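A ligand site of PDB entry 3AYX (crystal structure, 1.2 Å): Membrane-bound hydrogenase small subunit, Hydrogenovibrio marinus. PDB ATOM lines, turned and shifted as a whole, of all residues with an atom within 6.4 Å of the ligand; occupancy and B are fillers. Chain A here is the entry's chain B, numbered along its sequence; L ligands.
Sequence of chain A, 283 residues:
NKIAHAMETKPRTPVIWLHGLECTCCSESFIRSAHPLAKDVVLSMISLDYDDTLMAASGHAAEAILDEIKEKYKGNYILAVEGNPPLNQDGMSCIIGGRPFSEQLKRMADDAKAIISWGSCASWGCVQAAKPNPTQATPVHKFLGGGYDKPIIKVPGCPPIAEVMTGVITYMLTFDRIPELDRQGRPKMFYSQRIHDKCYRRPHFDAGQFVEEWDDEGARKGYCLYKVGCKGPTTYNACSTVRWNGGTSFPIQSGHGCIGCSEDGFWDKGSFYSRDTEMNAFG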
ATOM      1  N   ILE A 195      14.196 -31.549 -31.145  1.00  0.00           N
ATOM      2  CA  ILE A 195      13.928 -30.761 -29.949  1.00  0.00           C
ATOM      3  C   ILE A 195      14.736 -29.463 -30.032  1.00  0.00           C
ATOM      4  O   ILE A 195      14.218 -28.348 -29.845  1.00  0.00           O
ATOM      5  CB  ILE A 195      14.250 -31.509 -28.661  1.00  0.00           C
ATOM      6  CG1 ILE A 195      13.544 -32.847 -28.549  1.00  0.00           C
ATOM      7  CG2 ILE A 195      13.911 -30.607 -27.463  1.00  0.00           C
ATOM      8  CD1 ILE A 195      12.058 -32.712 -28.716  1.00  0.00           C
ATOM      9  N   HIS A 196      16.018 -29.563 -30.363  1.00  0.00           N
ATOM     10  CA  HIS A 196      17.016 -28.517 -30.384  1.00  0.00           C
ATOM     11  C   HIS A 196      16.758 -27.503 -31.531  1.00  0.00           C
ATOM     12  O   HIS A 196      17.291 -26.401 -31.526  1.00  0.00           O
ATOM     13  CB  HIS A 196      18.385 -29.145 -30.529  1.00  0.00           C
ATOM     14  CG  HIS A 196      19.621 -28.325 -30.496  1.00  0.00           C
ATOM     15  ND1 HIS A 196      20.145 -27.806 -29.339  1.00  0.00           N
ATOM     16  CD2 HIS A 196      20.477 -28.001 -31.501  1.00  0.00           C
ATOM     17  CE1 HIS A 196      21.290 -27.167 -29.671  1.00  0.00           C
ATOM     18  NE2 HIS A 196      21.493 -27.268 -30.980  1.00  0.00           N
ATOM     19  N   ASP A 197      15.949 -27.905 -32.519  1.00  0.00           N
ATOM     20  CA  ASP A 197      15.582 -26.996 -33.611  1.00  0.00           C
ATOM     21  C   ASP A 197      14.525 -26.019 -33.175  1.00  0.00           C
ATOM     22  O   ASP A 197      14.230 -25.109 -33.980  1.00  0.00           O
ATOM     23  CB  ASP A 197      15.068 -27.840 -34.786  1.00  0.00           C
ATOM     24  CG  ASP A 197      16.001 -28.678 -35.528  1.00  0.00           C
ATOM     25  OD1 ASP A 197      17.192 -28.358 -35.589  1.00  0.00           O
ATOM     26  OD2 ASP A 197      15.621 -29.740 -36.062  1.00  0.00           O
ATOM     27  N   CYS A 199      14.096 -25.176 -29.439  1.00  0.00           N
ATOM     28  CA  CYS A 199      14.244 -25.142 -27.976  1.00  0.00           C
ATOM     29  C   CYS A 199      14.478 -23.745 -27.489  1.00  0.00           C
ATOM     30  O   CYS A 199      15.404 -23.045 -27.917  1.00  0.00           O
ATOM     31  CB  CYS A 199      15.464 -26.013 -27.585  1.00  0.00           C
ATOM     32  SG  CYS A 199      15.602 -26.112 -25.764  1.00  0.00           S
ATOM     33  N   TYR A 200      13.656 -23.328 -26.556  1.00  0.00           N
ATOM     34  CA  TYR A 200      13.712 -22.000 -25.930  1.00  0.00           C
ATOM     35  C   TYR A 200      14.993 -21.787 -25.112  1.00  0.00           C
ATOM     36  O   TYR A 200      15.267 -20.633 -24.845  1.00  0.00           O
ATOM     37  CB  TYR A 200      12.429 -21.760 -25.069  1.00  0.00           C
ATOM     38  CG  TYR A 200      12.580 -22.359 -23.691  1.00  0.00           C
ATOM     39  CD1 TYR A 200      12.798 -21.587 -22.575  1.00  0.00           C
ATOM     40  CD2 TYR A 200      12.548 -23.737 -23.475  1.00  0.00           C
ATOM     41  CE1 TYR A 200      12.933 -22.068 -21.290  1.00  0.00           C
ATOM     42  CE2 TYR A 200      12.744 -24.255 -22.221  1.00  0.00           C
ATOM     43  CZ  TYR A 200      12.926 -23.448 -21.140  1.00  0.00           C
ATOM     44  OH  TYR A 200      13.176 -24.048 -19.909  1.00  0.00           O
ATOM     45  N   ARG A 201      15.758 -22.827 -24.803  1.00  0.00           N
ATOM     46  CA  ARG A 201      17.071 -22.645 -24.143  1.00  0.00           C
ATOM     47  C   ARG A 201      18.199 -22.446 -25.162  1.00  0.00           C
ATOM     48  O   ARG A 201      19.337 -22.173 -24.771  1.00  0.00           O
ATOM     49  CB  ARG A 201      17.439 -23.730 -23.154  1.00  0.00           C
ATOM     50  CG  ARG A 201      16.435 -23.883 -22.024  1.00  0.00           C
ATOM     51  CD  ARG A 201      17.016 -24.770 -20.923  1.00  0.00           C
ATOM     52  NE  ARG A 201      16.033 -24.911 -19.813  1.00  0.00           N
ATOM     53  CZ  ARG A 201      16.328 -25.194 -18.549  1.00  0.00           C
ATOM     54  NH1 ARG A 201      15.331 -25.306 -17.664  1.00  0.00           N
ATOM     55  NH2 ARG A 201      17.555 -25.343 -18.152  1.00  0.00           N
ATOM     56  N   ARG A 202      17.904 -22.527 -26.458  1.00  0.00           N
ATOM     57  CA  ARG A 202      18.909 -22.321 -27.492  1.00  0.00           C
ATOM     58  C   ARG A 202      19.701 -21.030 -27.355  1.00  0.00           C
ATOM     59  O   ARG A 202      20.916 -21.057 -27.603  1.00  0.00           O
ATOM     60  CB  ARG A 202      18.338 -22.426 -28.877  1.00  0.00           C
ATOM     61  CG  ARG A 202      19.337 -22.326 -30.020  1.00  0.00           C
ATOM     62  CD  ARG A 202      20.249 -23.598 -30.031  1.00  0.00           C
ATOM     63  NE  ARG A 202      21.023 -23.430 -31.276  1.00  0.00           N
ATOM     64  CZ  ARG A 202      20.775 -23.949 -32.474  1.00  0.00           C
ATOM     65  NH1 ARG A 202      19.742 -24.817 -32.601  1.00  0.00           N
ATOM     66  NH2 ARG A 202      21.567 -23.603 -33.413  1.00  0.00           N
ATOM     67  N   PRO A 203      19.100 -19.873 -26.995  1.00  0.00           N
ATOM     68  CA  PRO A 203      19.960 -18.674 -26.807  1.00  0.00           C
ATOM     69  C   PRO A 203      21.114 -18.910 -25.856  1.00  0.00           C
ATOM     70  O   PRO A 203      22.224 -18.409 -26.092  1.00  0.00           O
ATOM     71  CB  PRO A 203      18.982 -17.661 -26.239  1.00  0.00           C
ATOM     72  CG  PRO A 203      17.638 -18.104 -26.828  1.00  0.00           C
ATOM     73  CD  PRO A 203      17.683 -19.561 -26.770  1.00  0.00           C
ATOM     74  N   PHE A 205      22.566 -21.990 -25.239  1.00  0.00           N
ATOM     75  CA  PHE A 205      23.489 -22.875 -26.001  1.00  0.00           C
ATOM     76  C   PHE A 205      24.436 -22.010 -26.843  1.00  0.00           C
ATOM     77  O   PHE A 205      25.653 -22.163 -26.888  1.00  0.00           O
ATOM     78  CB  PHE A 205      22.714 -23.819 -26.871  1.00  0.00           C
ATOM     79  CG  PHE A 205      23.492 -24.748 -27.741  1.00  0.00           C
ATOM     80  CD1 PHE A 205      23.840 -24.355 -29.032  1.00  0.00           C
ATOM     81  CD2 PHE A 205      23.942 -25.978 -27.327  1.00  0.00           C
ATOM     82  CE1 PHE A 205      24.603 -25.156 -29.849  1.00  0.00           C
ATOM     83  CE2 PHE A 205      24.674 -26.829 -28.139  1.00  0.00           C
ATOM     84  CZ  PHE A 205      24.995 -26.413 -29.405  1.00  0.00           C
ATOM     85  N   PHE A 210      25.682 -22.778 -19.963  1.00  0.00           N
ATOM     86  CA  PHE A 210      25.244 -24.143 -19.664  1.00  0.00           C
ATOM     87  C   PHE A 210      25.100 -24.352 -18.193  1.00  0.00           C
ATOM     88  O   PHE A 210      25.804 -23.774 -17.338  1.00  0.00           O
ATOM     89  CB  PHE A 210      26.315 -25.140 -20.175  1.00  0.00           C
ATOM     90  CG  PHE A 210      26.618 -25.051 -21.609  1.00  0.00           C
ATOM     91  CD1 PHE A 210      25.655 -25.482 -22.530  1.00  0.00           C
ATOM     92  CD2 PHE A 210      27.832 -24.573 -22.062  1.00  0.00           C
ATOM     93  CE1 PHE A 210      25.930 -25.419 -23.846  1.00  0.00           C
ATOM     94  CE2 PHE A 210      28.107 -24.483 -23.413  1.00  0.00           C
ATOM     95  CZ  PHE A 210      27.134 -24.937 -24.318  1.00  0.00           C
ATOM     96  N   TYR A 223      19.702 -22.159 -18.096  1.00  0.00           N
ATOM     97  CA  TYR A 223      20.763 -22.347 -19.106  1.00  0.00           C
ATOM     98  C   TYR A 223      20.631 -23.679 -19.774  1.00  0.00           C
ATOM     99  O   TYR A 223      19.958 -24.594 -19.325  1.00  0.00           O
ATOM    100  CB  TYR A 223      22.140 -22.157 -18.453  1.00  0.00           C
ATOM    101  CG  TYR A 223      22.560 -20.735 -18.179  1.00  0.00           C
ATOM    102  CD1 TYR A 223      21.763 -19.648 -18.299  1.00  0.00           C
ATOM    103  CD2 TYR A 223      23.891 -20.538 -17.733  1.00  0.00           C
ATOM    104  CE1 TYR A 223      22.235 -18.403 -18.025  1.00  0.00           C
ATOM    105  CE2 TYR A 223      24.372 -19.254 -17.445  1.00  0.00           C
ATOM    106  CZ  TYR A 223      23.536 -18.163 -17.595  1.00  0.00           C
ATOM    107  OH  TYR A 223      24.007 -16.888 -17.310  1.00  0.00           O
ATOM    108  N   CYS A 224      21.293 -23.804 -20.922  1.00  0.00           N
ATOM    109  CA  CYS A 224      21.189 -25.001 -21.746  1.00  0.00           C
ATOM    110  C   CYS A 224      21.697 -26.217 -20.976  1.00  0.00           C
ATOM    111  O   CYS A 224      22.660 -26.139 -20.197  1.00  0.00           O
ATOM    112  CB  CYS A 224      22.019 -24.740 -23.021  1.00  0.00           C
ATOM    113  SG  CYS A 224      22.271 -26.220 -24.065  1.00  0.00           S
ATOM    114  N   LEU A 225      21.073 -27.346 -21.249  1.00  0.00           N
ATOM    115  CA  LEU A 225      21.306 -28.660 -20.623  1.00  0.00           C
ATOM    116  C   LEU A 225      22.220 -29.547 -21.381  1.00  0.00           C
ATOM    117  O   LEU A 225      22.445 -30.715 -21.027  1.00  0.00           O
ATOM    118  CB  LEU A 225      19.964 -29.346 -20.320  1.00  0.00           C
ATOM    119  CG  LEU A 225      19.054 -28.536 -19.405  1.00  0.00           C
ATOM    120  CD1 LEU A 225      17.677 -29.119 -19.381  1.00  0.00           C
ATOM    121  CD2 LEU A 225      19.659 -28.458 -18.008  1.00  0.00           C
ATOM    122  N   TYR A 226      22.916 -29.051 -22.421  1.00  0.00           N
ATOM    123  CA  TYR A 226      23.807 -29.858 -23.257  1.00  0.00           C
ATOM    124  C   TYR A 226      24.865 -30.548 -22.415  1.00  0.00           C
ATOM    125  O   TYR A 226      25.202 -31.737 -22.635  1.00  0.00           O
ATOM    126  CB  TYR A 226      24.454 -28.983 -24.386  1.00  0.00           C
ATOM    127  CG  TYR A 226      25.418 -29.836 -25.164  1.00  0.00           C
ATOM    128  CD1 TYR A 226      24.987 -30.729 -26.120  1.00  0.00           C
ATOM    129  CD2 TYR A 226      26.780 -29.797 -24.915  1.00  0.00           C
ATOM    130  CE1 TYR A 226      25.827 -31.538 -26.830  1.00  0.00           C
ATOM    131  CE2 TYR A 226      27.655 -30.640 -25.591  1.00  0.00           C
ATOM    132  CZ  TYR A 226      27.161 -31.475 -26.556  1.00  0.00           C
ATOM    133  OH  TYR A 226      28.057 -32.298 -27.181  1.00  0.00           O
ATOM    134  N   LYS A 227      25.523 -29.828 -21.517  1.00  0.00           N
ATOM    135  CA  LYS A 227      26.652 -30.402 -20.801  1.00  0.00           C
ATOM    136  C   LYS A 227      26.226 -31.436 -19.760  1.00  0.00           C
ATOM    137  O   LYS A 227      27.075 -32.229 -19.373  1.00  0.00           O
ATOM    138  CB  LYS A 227      27.487 -29.324 -20.140  1.00  0.00           C
ATOM    139  CG  LYS A 227      28.249 -28.455 -21.125  1.00  0.00           C
ATOM    140  CD  LYS A 227      29.259 -27.525 -20.525  1.00  0.00           C
ATOM    141  CE  LYS A 227      30.675 -27.602 -20.991  1.00  0.00           C
ATOM    142  NZ  LYS A 227      31.455 -26.707 -20.109  1.00  0.00           N
ATOM    143  N   CYS A 230      21.751 -33.432 -22.403  1.00  0.00           N
ATOM    144  CA  CYS A 230      20.575 -33.294 -23.261  1.00  0.00           C
ATOM    145  C   CYS A 230      20.785 -33.904 -24.680  1.00  0.00           C
ATOM    146  O   CYS A 230      21.763 -33.559 -25.352  1.00  0.00           O
ATOM    147  CB  CYS A 230      20.278 -31.796 -23.349  1.00  0.00           C
ATOM    148  SG  CYS A 230      18.690 -31.532 -24.293  1.00  0.00           S
ATOM    149  N   LYS A 231      19.844 -34.747 -25.049  1.00  0.00           N
ATOM    150  CA  LYS A 231      19.835 -35.385 -26.372  1.00  0.00           C
ATOM    151  C   LYS A 231      18.946 -34.687 -27.354  1.00  0.00           C
ATOM    152  O   LYS A 231      18.707 -35.180 -28.473  1.00  0.00           O
ATOM    153  CB  LYS A 231      19.553 -36.862 -26.271  1.00  0.00           C
ATOM    154  CG  LYS A 231      20.473 -37.635 -25.379  1.00  0.00           C
ATOM    155  CD  LYS A 231      21.857 -37.684 -25.873  1.00  0.00           C
ATOM    156  CE  LYS A 231      23.009 -37.762 -24.989  1.00  0.00           C
ATOM    157  NZ  LYS A 231      22.871 -38.125 -23.602  1.00  0.00           N
ATOM    158  N   GLY A 232      18.520 -33.488 -27.032  1.00  0.00           N
ATOM    159  CA  GLY A 232      17.692 -32.693 -27.938  1.00  0.00           C
ATOM    160  C   GLY A 232      18.346 -32.475 -29.268  1.00  0.00           C
ATOM    161  O   GLY A 232      17.575 -32.468 -30.286  1.00  0.00           O
ATOM    162  N   PRO A 233      19.648 -32.297 -29.401  1.00  0.00           N
ATOM    163  CA  PRO A 233      20.279 -32.114 -30.747  1.00  0.00           C
ATOM    164  C   PRO A 233      20.046 -33.264 -31.698  1.00  0.00           C
ATOM    165  O   PRO A 233      20.208 -33.023 -32.907  1.00  0.00           O
ATOM    166  CB  PRO A 233      21.755 -31.914 -30.446  1.00  0.00           C
ATOM    167  CG  PRO A 233      21.718 -31.278 -29.031  1.00  0.00           C
ATOM    168  CD  PRO A 233      20.642 -32.031 -28.332  1.00  0.00           C
ATOM    169  N   PHE A 250       7.925 -29.515 -20.629  1.00  0.00           N
ATOM    170  CA  PHE A 250       8.579 -30.623 -21.302  1.00  0.00           C
ATOM    171  C   PHE A 250       9.878 -30.899 -20.491  1.00  0.00           C
ATOM    172  O   PHE A 250      10.223 -30.116 -19.623  1.00  0.00           O
ATOM    173  CB  PHE A 250       8.807 -30.378 -22.770  1.00  0.00           C
ATOM    174  CG  PHE A 250       9.823 -29.395 -23.228  1.00  0.00           C
ATOM    175  CD1 PHE A 250      10.943 -29.730 -23.956  1.00  0.00           C
ATOM    176  CD2 PHE A 250       9.660 -28.026 -23.009  1.00  0.00           C
ATOM    177  CE1 PHE A 250      11.826 -28.868 -24.510  1.00  0.00           C
ATOM    178  CE2 PHE A 250      10.560 -27.101 -23.548  1.00  0.00           C
ATOM    179  CZ  PHE A 250      11.664 -27.491 -24.285  1.00  0.00           C
ATOM    180  N   ILE A 252      13.102 -30.525 -20.715  1.00  0.00           N
ATOM    181  CA  ILE A 252      14.066 -29.449 -20.653  1.00  0.00           C
ATOM    182  C   ILE A 252      13.526 -28.282 -19.836  1.00  0.00           C
ATOM    183  O   ILE A 252      14.266 -27.697 -19.044  1.00  0.00           O
ATOM    184  CB  ILE A 252      14.471 -29.045 -22.080  1.00  0.00           C
ATOM    185  CG1 ILE A 252      15.337 -30.159 -22.693  1.00  0.00           C
ATOM    186  CG2 ILE A 252      15.118 -27.670 -22.131  1.00  0.00           C
ATOM    187  CD1 ILE A 252      15.141 -30.394 -24.139  1.00  0.00           C
ATOM    188  N   GLY A 257      17.837 -32.801 -19.182  1.00  0.00           N
ATOM    189  CA  GLY A 257      17.958 -32.938 -20.606  1.00  0.00           C
ATOM    190  C   GLY A 257      17.004 -33.970 -21.187  1.00  0.00           C
ATOM    191  O   GLY A 257      16.612 -34.953 -20.521  1.00  0.00           O
ATOM    192  N   CYS A 258      16.680 -33.810 -22.453  1.00  0.00           N
ATOM    193  CA  CYS A 258      16.107 -34.872 -23.267  1.00  0.00           C
ATOM    194  C   CYS A 258      16.970 -36.117 -23.110  1.00  0.00           C
ATOM    195  O   CYS A 258      18.211 -36.031 -23.133  1.00  0.00           O
ATOM    196  CB  CYS A 258      16.013 -34.355 -24.685  1.00  0.00           C
ATOM    197  SG  CYS A 258      15.402 -35.537 -25.936  1.00  0.00           S
ATOM    198  N   MET A 279      27.834 -32.670 -33.107  1.00  0.00           N
ATOM    199  CA  MET A 279      27.492 -31.265 -32.912  1.00  0.00           C
ATOM    200  C   MET A 279      28.200 -30.299 -33.846  1.00  0.00           C
ATOM    201  O   MET A 279      27.712 -29.169 -34.035  1.00  0.00           O
ATOM    202  CB  MET A 279      27.784 -30.877 -31.499  1.00  0.00           C
ATOM    203  CG  MET A 279      26.997 -31.656 -30.475  1.00  0.00           C
ATOM    204  SD  MET A 279      25.256 -31.637 -30.495  1.00  0.00           S
ATOM    205  CE  MET A 279      25.005 -29.921 -30.014  1.00  0.00           C
HETATM  206 FE1  LIG L   1      17.682 -27.066 -25.653  1.00  0.00          FE
HETATM  207 FE2  LIG L   1      20.327 -26.994 -24.970  1.00  0.00          FE
HETATM  208 FE3  LIG L   1      18.971 -29.402 -25.135  1.00  0.00          FE
HETATM  209 FE4  LIG L   1      19.539 -27.970 -27.349  1.00  0.00          FE
HETATM  210  S1  LIG L   1      21.056 -28.977 -25.972  1.00  0.00           S
HETATM  211  S2  LIG L   1      17.585 -29.034 -26.920  1.00  0.00           S
HETATM  212  S3  LIG L   1      19.318 -25.791 -26.613  1.00  0.00           S
HETATM  213  S4  LIG L   1      18.591 -27.653 -23.644  1.00  0.00           S
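N of Leu 225 lies close to S4 of the ligand, 3.5 Å away. The side-chain sulfur (SG) of Cys 230 binds an iron atom (FE3) of the ligand (2.3 Å). The side-chain sulfur of Cys 199 binds an iron atom (FE1) of the ligand (2.3 Å). The side-chain sulfur (SG) of Cys 224 binds an iron atom (FE2) of the ligand (2.3 Å). A ring nitrogen (ND1) of His 196 is bound to an iron atom (FE4) of the ligand, 2.1 Å away. A sulfur (S3) of the ligand lies close to the backbone NH (N) of Arg 202 (3.6 Å).
Residues that only touch the ligand: Tyr 226, Ile 252, Gly 232, Arg 201, Pro 233 and Phe 205. 12 residues have an atom within 4 Å of the ligand: His 196, Cys 199, Arg 201, Arg 202, Phe 205, Cys 224, Leu 225, Tyr 226, Cys 230, Gly 232, Pro 233 and Ile 252. The nearest printed residue that does not touch the ligand is Ile 195 (4.03 Å).
The backbone NH (N) of Tyr 226 sits close to the side-chain sulfur (SG) of Cys 224, 3.3 Å away. NH2 of Arg 201 lies within hydrogen-bond range of O of Tyr 223, 2.8 Å away. The guanidinium group (NE) of Arg 201 sits at hydrogen-bond distance from the side-chain hydroxyl (OH) of Tyr 200 (3.0 Å). The backbone NH (N) of Cys 258 lies close to the side-chain sulfur (SG) of Cys 230 (3.6 Å). N of Cys 230 sits at hydrogen-bond distance from O of Leu 225 (3.1 Å). NH1 of Arg 202 sits at hydrogen-bond distance from O of His 196 (3.1 Å). SG of Cys 230 sits close to N of Gly 232, 3.4 Å away. O of Gly 232 lies within hydrogen-bond range of N of His 196 (3.3 Å).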
